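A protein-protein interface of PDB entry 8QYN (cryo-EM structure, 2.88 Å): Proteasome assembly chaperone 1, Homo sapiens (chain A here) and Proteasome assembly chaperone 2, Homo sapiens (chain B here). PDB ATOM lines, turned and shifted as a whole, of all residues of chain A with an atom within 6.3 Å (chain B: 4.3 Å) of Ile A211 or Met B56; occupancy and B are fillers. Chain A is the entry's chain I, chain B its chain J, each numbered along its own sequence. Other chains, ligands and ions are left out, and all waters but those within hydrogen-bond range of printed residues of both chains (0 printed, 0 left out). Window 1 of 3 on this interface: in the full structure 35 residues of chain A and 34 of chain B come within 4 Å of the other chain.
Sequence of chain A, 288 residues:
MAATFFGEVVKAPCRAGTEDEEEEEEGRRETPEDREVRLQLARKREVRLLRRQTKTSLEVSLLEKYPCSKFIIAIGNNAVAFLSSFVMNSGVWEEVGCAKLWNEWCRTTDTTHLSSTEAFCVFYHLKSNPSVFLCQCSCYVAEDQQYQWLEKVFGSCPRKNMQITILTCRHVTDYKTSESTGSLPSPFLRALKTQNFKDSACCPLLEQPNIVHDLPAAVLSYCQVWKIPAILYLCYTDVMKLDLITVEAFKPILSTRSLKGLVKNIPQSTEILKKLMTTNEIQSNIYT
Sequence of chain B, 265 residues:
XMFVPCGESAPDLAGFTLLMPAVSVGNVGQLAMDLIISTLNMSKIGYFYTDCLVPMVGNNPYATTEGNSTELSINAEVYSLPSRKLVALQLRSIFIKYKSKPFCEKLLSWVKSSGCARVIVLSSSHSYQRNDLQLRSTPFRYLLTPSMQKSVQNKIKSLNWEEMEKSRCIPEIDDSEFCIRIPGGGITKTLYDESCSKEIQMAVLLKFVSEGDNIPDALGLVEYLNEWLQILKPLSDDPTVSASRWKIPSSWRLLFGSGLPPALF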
ATOM      1  N   ASP A 174      27.079  25.195 -18.232  1.00  0.00           N
ATOM      2  CA  ASP A 174      26.032  24.190 -18.344  1.00  0.00           C
ATOM      3  C   ASP A 174      25.195  24.347 -19.605  1.00  0.00           C
ATOM      4  O   ASP A 174      24.293  23.537 -19.835  1.00  0.00           O
ATOM      5  CB  ASP A 174      25.121  24.243 -17.116  1.00  0.00           C
ATOM      6  CG  ASP A 174      25.842  23.862 -15.843  1.00  0.00           C
ATOM      7  OD1 ASP A 174      27.062  23.606 -15.905  1.00  0.00           O
ATOM      8  OD2 ASP A 174      25.191  23.817 -14.778  1.00  0.00           O
ATOM      9  N   LEU A 192      11.055  29.344 -19.609  1.00  0.00           N
ATOM     10  CA  LEU A 192      10.305  28.105 -19.787  1.00  0.00           C
ATOM     11  C   LEU A 192       8.954  28.292 -19.119  1.00  0.00           C
ATOM     12  O   LEU A 192       8.899  28.592 -17.924  1.00  0.00           O
ATOM     13  CB  LEU A 192      11.039  26.912 -19.176  1.00  0.00           C
ATOM     14  CG  LEU A 192      12.073  26.176 -20.025  1.00  0.00           C
ATOM     15  CD1 LEU A 192      12.805  25.157 -19.180  1.00  0.00           C
ATOM     16  CD2 LEU A 192      11.410  25.505 -21.203  1.00  0.00           C
ATOM     17  N   LEU A 206      14.082  28.475 -23.884  1.00  0.00           N
ATOM     18  CA  LEU A 206      15.276  27.645 -23.814  1.00  0.00           C
ATOM     19  C   LEU A 206      15.357  26.712 -25.015  1.00  0.00           C
ATOM     20  O   LEU A 206      14.344  26.192 -25.489  1.00  0.00           O
ATOM     21  CB  LEU A 206      15.282  26.838 -22.519  1.00  0.00           C
ATOM     22  CG  LEU A 206      16.614  26.221 -22.094  1.00  0.00           C
ATOM     23  CD1 LEU A 206      17.689  27.279 -21.996  1.00  0.00           C
ATOM     24  CD2 LEU A 206      16.464  25.488 -20.779  1.00  0.00           C
ATOM     25  N   GLU A 207      16.576  26.499 -25.505  1.00  0.00           N
ATOM     26  CA  GLU A 207      16.795  25.631 -26.651  1.00  0.00           C
ATOM     27  C   GLU A 207      16.464  24.187 -26.279  1.00  0.00           C
ATOM     28  O   GLU A 207      16.142  23.868 -25.134  1.00  0.00           O
ATOM     29  CB  GLU A 207      18.231  25.767 -27.145  1.00  0.00           C
ATOM     30  CG  GLU A 207      18.429  26.908 -28.124  1.00  0.00           C
ATOM     31  CD  GLU A 207      18.274  28.266 -27.467  1.00  0.00           C
ATOM     32  OE1 GLU A 207      18.585  28.380 -26.265  1.00  0.00           O
ATOM     33  OE2 GLU A 207      17.838  29.217 -28.149  1.00  0.00           O
ATOM     34  N   GLN A 208      16.536  23.299 -27.265  1.00  0.00           N
ATOM     35  CA  GLN A 208      16.031  21.950 -27.036  1.00  0.00           C
ATOM     36  C   GLN A 208      16.940  21.120 -26.132  1.00  0.00           C
ATOM     37  O   GLN A 208      16.534  20.807 -25.007  1.00  0.00           O
ATOM     38  CB  GLN A 208      15.785  21.233 -28.362  1.00  0.00           C
ATOM     39  CG  GLN A 208      14.702  21.887 -29.187  1.00  0.00           C
ATOM     40  CD  GLN A 208      13.373  21.903 -28.468  1.00  0.00           C
ATOM     41  OE1 GLN A 208      13.023  20.956 -27.770  1.00  0.00           O
ATOM     42  NE2 GLN A 208      12.624  22.982 -28.633  1.00  0.00           N
ATOM     43  N   PRO A 209      18.177  20.775 -26.535  1.00  0.00           N
ATOM     44  CA  PRO A 209      18.911  19.741 -25.787  1.00  0.00           C
ATOM     45  C   PRO A 209      19.238  20.129 -24.353  1.00  0.00           C
ATOM     46  O   PRO A 209      19.821  19.334 -23.612  1.00  0.00           O
ATOM     47  CB  PRO A 209      20.182  19.549 -26.617  1.00  0.00           C
ATOM     48  CG  PRO A 209      20.396  20.847 -27.259  1.00  0.00           C
ATOM     49  CD  PRO A 209      19.040  21.423 -27.538  1.00  0.00           C
ATOM     50  N   ASN A 210      18.857  21.337 -23.947  1.00  0.00           N
ATOM     51  CA  ASN A 210      19.097  21.818 -22.595  1.00  0.00           C
ATOM     52  C   ASN A 210      17.921  21.483 -21.688  1.00  0.00           C
ATOM     53  O   ASN A 210      16.760  21.619 -22.079  1.00  0.00           O
ATOM     54  CB  ASN A 210      19.326  23.328 -22.599  1.00  0.00           C
ATOM     55  CG  ASN A 210      20.650  23.707 -23.202  1.00  0.00           C
ATOM     56  OD1 ASN A 210      21.701  23.468 -22.615  1.00  0.00           O
ATOM     57  ND2 ASN A 210      20.612  24.303 -24.385  1.00  0.00           N
ATOM     58  N   ILE A 211      18.234  21.047 -20.468  1.00  0.00           N
ATOM     59  CA  ILE A 211      17.235  20.747 -19.452  1.00  0.00           C
ATOM     60  C   ILE A 211      17.636  21.440 -18.158  1.00  0.00           C
ATOM     61  O   ILE A 211      18.779  21.860 -17.978  1.00  0.00           O
ATOM     62  CB  ILE A 211      17.069  19.232 -19.212  1.00  0.00           C
ATOM     63  CG1 ILE A 211      18.383  18.625 -18.729  1.00  0.00           C
ATOM     64  CG2 ILE A 211      16.587  18.539 -20.468  1.00  0.00           C
ATOM     65  CD1 ILE A 211      18.223  17.283 -18.072  1.00  0.00           C
ATOM     66  N   VAL A 212      16.669  21.561 -17.255  1.00  0.00           N
ATOM     67  CA  VAL A 212      16.883  22.142 -15.937  1.00  0.00           C
ATOM     68  C   VAL A 212      16.310  21.193 -14.893  1.00  0.00           C
ATOM     69  O   VAL A 212      15.256  20.585 -15.107  1.00  0.00           O
ATOM     70  CB  VAL A 212      16.254  23.548 -15.826  1.00  0.00           C
ATOM     71  CG1 VAL A 212      14.754  23.490 -16.027  1.00  0.00           C
ATOM     72  CG2 VAL A 212      16.584  24.178 -14.487  1.00  0.00           C
ATOM     73  N   HIS A 213      17.020  21.041 -13.775  1.00  0.00           N
ATOM     74  CA  HIS A 213      16.571  20.137 -12.723  1.00  0.00           C
ATOM     75  C   HIS A 213      16.559  20.824 -11.361  1.00  0.00           C
ATOM     76  O   HIS A 213      16.717  22.045 -11.278  1.00  0.00           O
ATOM     77  CB  HIS A 213      17.444  18.880 -12.684  1.00  0.00           C
ATOM     78  CG  HIS A 213      18.879  19.140 -12.347  1.00  0.00           C
ATOM     79  ND1 HIS A 213      19.695  19.932 -13.125  1.00  0.00           N
ATOM     80  CD2 HIS A 213      19.647  18.698 -11.325  1.00  0.00           C
ATOM     81  CE1 HIS A 213      20.903  19.975 -12.589  1.00  0.00           C
ATOM     82  NE2 HIS A 213      20.900  19.234 -11.497  1.00  0.00           N
ATOM     83  N   ASP A 214      16.349  20.036 -10.303  1.00  0.00           N
ATOM     84  CA  ASP A 214      16.269  20.483  -8.912  1.00  0.00           C
ATOM     85  C   ASP A 214      14.975  21.236  -8.622  1.00  0.00           C
ATOM     86  O   ASP A 214      13.962  21.012  -9.290  1.00  0.00           O
ATOM     87  CB  ASP A 214      17.484  21.337  -8.538  1.00  0.00           C
ATOM     88  CG  ASP A 214      18.610  20.517  -7.944  1.00  0.00           C
ATOM     89  OD1 ASP A 214      18.378  19.331  -7.626  1.00  0.00           O
ATOM     90  OD2 ASP A 214      19.728  21.054  -7.797  1.00  0.00           O
ATOM     91  N   ALA A 217      12.604  22.976 -11.180  1.00  0.00           N
ATOM     92  CA  ALA A 217      12.003  21.933 -11.999  1.00  0.00           C
ATOM     93  C   ALA A 217      10.862  21.249 -11.261  1.00  0.00           C
ATOM     94  O   ALA A 217       9.842  20.907 -11.866  1.00  0.00           O
ATOM     95  CB  ALA A 217      13.061  20.916 -12.414  1.00  0.00           C
ATOM     96  N   ALA A 218      11.017  21.040  -9.952  1.00  0.00           N
ATOM     97  CA  ALA A 218       9.940  20.447  -9.166  1.00  0.00           C
ATOM     98  C   ALA A 218       8.708  21.339  -9.157  1.00  0.00           C
ATOM     99  O   ALA A 218       7.577  20.857  -9.314  1.00  0.00           O
ATOM    100  CB  ALA A 218      10.417  20.179  -7.740  1.00  0.00           C
ATOM    101  N   SER A 221       7.062  21.173 -12.573  1.00  0.00           N
ATOM    102  CA  SER A 221       6.380  19.902 -12.777  1.00  0.00           C
ATOM    103  C   SER A 221       5.055  19.871 -12.028  1.00  0.00           C
ATOM    104  O   SER A 221       4.034  19.436 -12.576  1.00  0.00           O
ATOM    105  CB  SER A 221       7.276  18.749 -12.336  1.00  0.00           C
ATOM    106  OG  SER A 221       8.567  18.872 -12.902  1.00  0.00           O
ATOM    107  N   TYR A 236      22.104  32.606 -17.190  1.00  0.00           N
ATOM    108  CA  TYR A 236      23.377  31.922 -17.386  1.00  0.00           C
ATOM    109  C   TYR A 236      24.490  32.960 -17.312  1.00  0.00           C
ATOM    110  O   TYR A 236      24.596  33.826 -18.184  1.00  0.00           O
ATOM    111  CB  TYR A 236      23.396  31.186 -18.722  1.00  0.00           C
ATOM    112  CG  TYR A 236      22.498  29.971 -18.770  1.00  0.00           C
ATOM    113  CD1 TYR A 236      22.969  28.726 -18.391  1.00  0.00           C
ATOM    114  CD2 TYR A 236      21.184  30.070 -19.197  1.00  0.00           C
ATOM    115  CE1 TYR A 236      22.158  27.616 -18.433  1.00  0.00           C
ATOM    116  CE2 TYR A 236      20.367  28.963 -19.243  1.00  0.00           C
ATOM    117  CZ  TYR A 236      20.860  27.740 -18.858  1.00  0.00           C
ATOM    118  OH  TYR A 236      20.052  26.629 -18.899  1.00  0.00           O
ATOM    119  N   VAL B  54      13.828  11.916  -9.654  1.00  0.00           N
ATOM    120  CA  VAL B  54      14.352  13.283  -9.555  1.00  0.00           C
ATOM    121  C   VAL B  54      13.692  14.150 -10.623  1.00  0.00           C
ATOM    122  O   VAL B  54      13.730  13.794 -11.812  1.00  0.00           O
ATOM    123  CB  VAL B  54      15.872  13.281  -9.711  1.00  0.00           C
ATOM    124  CG1 VAL B  54      16.420  14.685  -9.566  1.00  0.00           C
ATOM    125  CG2 VAL B  54      16.505  12.360  -8.690  1.00  0.00           C
ATOM    126  N   PRO B  55      13.083  15.275 -10.260  1.00  0.00           N
ATOM    127  CA  PRO B  55      12.359  16.077 -11.251  1.00  0.00           C
ATOM    128  C   PRO B  55      13.286  16.732 -12.265  1.00  0.00           C
ATOM    129  O   PRO B  55      14.433  17.072 -11.970  1.00  0.00           O
ATOM    130  CB  PRO B  55      11.641  17.127 -10.400  1.00  0.00           C
ATOM    131  CG  PRO B  55      12.455  17.225  -9.163  1.00  0.00           C
ATOM    132  CD  PRO B  55      13.004  15.858  -8.910  1.00  0.00           C
ATOM    133  N   MET B  56      12.764  16.909 -13.477  1.00  0.00           N
ATOM    134  CA  MET B  56      13.475  17.592 -14.548  1.00  0.00           C
ATOM    135  C   MET B  56      12.454  18.135 -15.535  1.00  0.00           C
ATOM    136  O   MET B  56      11.348  17.604 -15.662  1.00  0.00           O
ATOM    137  CB  MET B  56      14.492  16.665 -15.232  1.00  0.00           C
ATOM    138  CG  MET B  56      13.918  15.423 -15.902  1.00  0.00           C
ATOM    139  SD  MET B  56      13.173  15.686 -17.520  1.00  0.00           S
ATOM    140  CE  MET B  56      14.625  16.012 -18.508  1.00  0.00           C
ATOM    141  N   VAL B  57      12.829  19.213 -16.221  1.00  0.00           N
ATOM    142  CA  VAL B  57      11.931  19.927 -17.123  1.00  0.00           C
ATOM    143  C   VAL B  57      12.695  20.341 -18.374  1.00  0.00           C
ATOM    144  O   VAL B  57      13.858  20.750 -18.298  1.00  0.00           O
ATOM    145  CB  VAL B  57      11.302  21.155 -16.430  1.00  0.00           C
ATOM    146  CG1 VAL B  57      10.550  22.002 -17.422  1.00  0.00           C
ATOM    147  CG2 VAL B  57      10.362  20.718 -15.328  1.00  0.00           C
ATOM    148  N   SER B  73       7.681  19.454 -20.907  1.00  0.00           N
ATOM    149  CA  SER B  73       7.708  18.029 -20.627  1.00  0.00           C
ATOM    150  C   SER B  73       8.262  17.806 -19.228  1.00  0.00           C
ATOM    151  O   SER B  73       9.029  18.622 -18.714  1.00  0.00           O
ATOM    152  CB  SER B  73       8.554  17.272 -21.654  1.00  0.00           C
ATOM    153  OG  SER B  73       9.933  17.395 -21.357  1.00  0.00           O
ATOM    154  N   ILE B  74       7.867  16.693 -18.616  1.00  0.00           N
ATOM    155  CA  ILE B  74       8.346  16.338 -17.286  1.00  0.00           C
ATOM    156  C   ILE B  74       9.022  14.975 -17.355  1.00  0.00           C
ATOM    157  O   ILE B  74       9.152  14.391 -18.436  1.00  0.00           O
ATOM    158  CB  ILE B  74       7.206  16.356 -16.252  1.00  0.00           C
ATOM    159  CG1 ILE B  74       6.240  15.198 -16.487  1.00  0.00           C
ATOM    160  CG2 ILE B  74       6.465  17.679 -16.307  1.00  0.00           C
ATOM    161  CD1 ILE B  74       5.340  14.921 -15.311  1.00  0.00           C
ATOM    162  N   ASN B  75       9.467  14.460 -16.207  1.00  0.00           N
ATOM    163  CA  ASN B  75      10.296  13.261 -16.187  1.00  0.00           C
ATOM    164  C   ASN B  75       9.531  11.977 -16.493  1.00  0.00           C
ATOM    165  O   ASN B  75      10.168  10.931 -16.650  1.00  0.00           O
ATOM    166  CB  ASN B  75      10.993  13.126 -14.834  1.00  0.00           C
ATOM    167  CG  ASN B  75      10.020  13.101 -13.680  1.00  0.00           C
ATOM    168  OD1 ASN B  75       8.860  13.476 -13.824  1.00  0.00           O
ATOM    169  ND2 ASN B  75      10.489  12.660 -12.521  1.00  0.00           N
ATOM    170  N   ARG B  92      12.722   9.848 -17.949  1.00  0.00           N
ATOM    171  CA  ARG B  92      13.891  10.626 -18.340  1.00  0.00           C
ATOM    172  C   ARG B  92      14.697  11.098 -17.136  1.00  0.00           C
ATOM    173  O   ARG B  92      15.275  12.184 -17.162  1.00  0.00           O
ATOM    174  CB  ARG B  92      13.481  11.824 -19.193  1.00  0.00           C
ATOM    175  CG  ARG B  92      12.708  11.466 -20.439  1.00  0.00           C
ATOM    176  CD  ARG B  92      12.677  12.626 -21.412  1.00  0.00           C
ATOM    177  NE  ARG B  92      11.634  12.461 -22.416  1.00  0.00           N
ATOM    178  CZ  ARG B  92      10.351  12.720 -22.209  1.00  0.00           C
ATOM    179  NH1 ARG B  92       9.916  13.166 -21.042  1.00  0.00           N
ATOM    180  NH2 ARG B  92       9.483  12.528 -23.196  1.00  0.00           N
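Of chain B, only Met B56 and Val B57 come within 4 Å of Ile A211. Of the printed residues of chain B, Ala A217 touches Met B56 (3.97 Å) and Val B57 (3.5 Å). Of the printed residues of chain B, Ala A218 touches Pro B55. Of chain A, only Ile A211, Val A212 and Ala A217 come within 4 Å of Met B56. Of the printed residues of chain A, Val B57 touches Ile A211 (3.6 Å), Val A212 (3.0 Å), Ala A217 (3.5 Å) and Ser A221 (3.5 Å). The nearest printed residue of chain B that does not touch His A213 is Met B56 (4.4 Å).
Of the 15 printed residues of chain A, 7 touch a printed residue of chain B. Printed residues of chain A that touch a printed residue of chain B: Ile A211, Val A212, His A213, Asp A214, Ala A217, Ala A218 and Ser A221. Hydrophobic or aromatic side chains of chain A within 4 Å of the printed part of chain B: Ile A211, Val A212, His A213, Ala A217 and Ala A218. Printed residues of chain B that touch a printed residue of chain A: Pro B55, Met B56 and Val B57. Hydrophobic or aromatic side chains of chain B that line the printed part of chain A: Pro B55, Met B56 and Val B57. Among the printed residues, no Asp or Glu carboxylate lies within 4 Å of a Lys or Arg side-chain nitrogen of the other chain.
Among the printed residues, merely in contact across the chains: Ile A211 with Met B56 (3.8 Å), Ile A211 with Val B57 (3.6 Å), Val A212 with Met B56 (3.5 Å), His A213 with Pro B55 (3.6 Å), Asp A214 with Pro B55 (3.9 Å), Ala A217 with Met B56 (3.97 Å), Ala A217 with Val B57 (3.5 Å), Ala A218 with Pro B55 (3.9 Å) and Ser A221 with Val B57 (3.5 Å).
O of Ala A217 is in hydrogen-bond range of OG of Ser A221 (2.6 Å).
N of Val B57 sits at hydrogen-bond distance from O of Val A212, 3.0 Å away.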
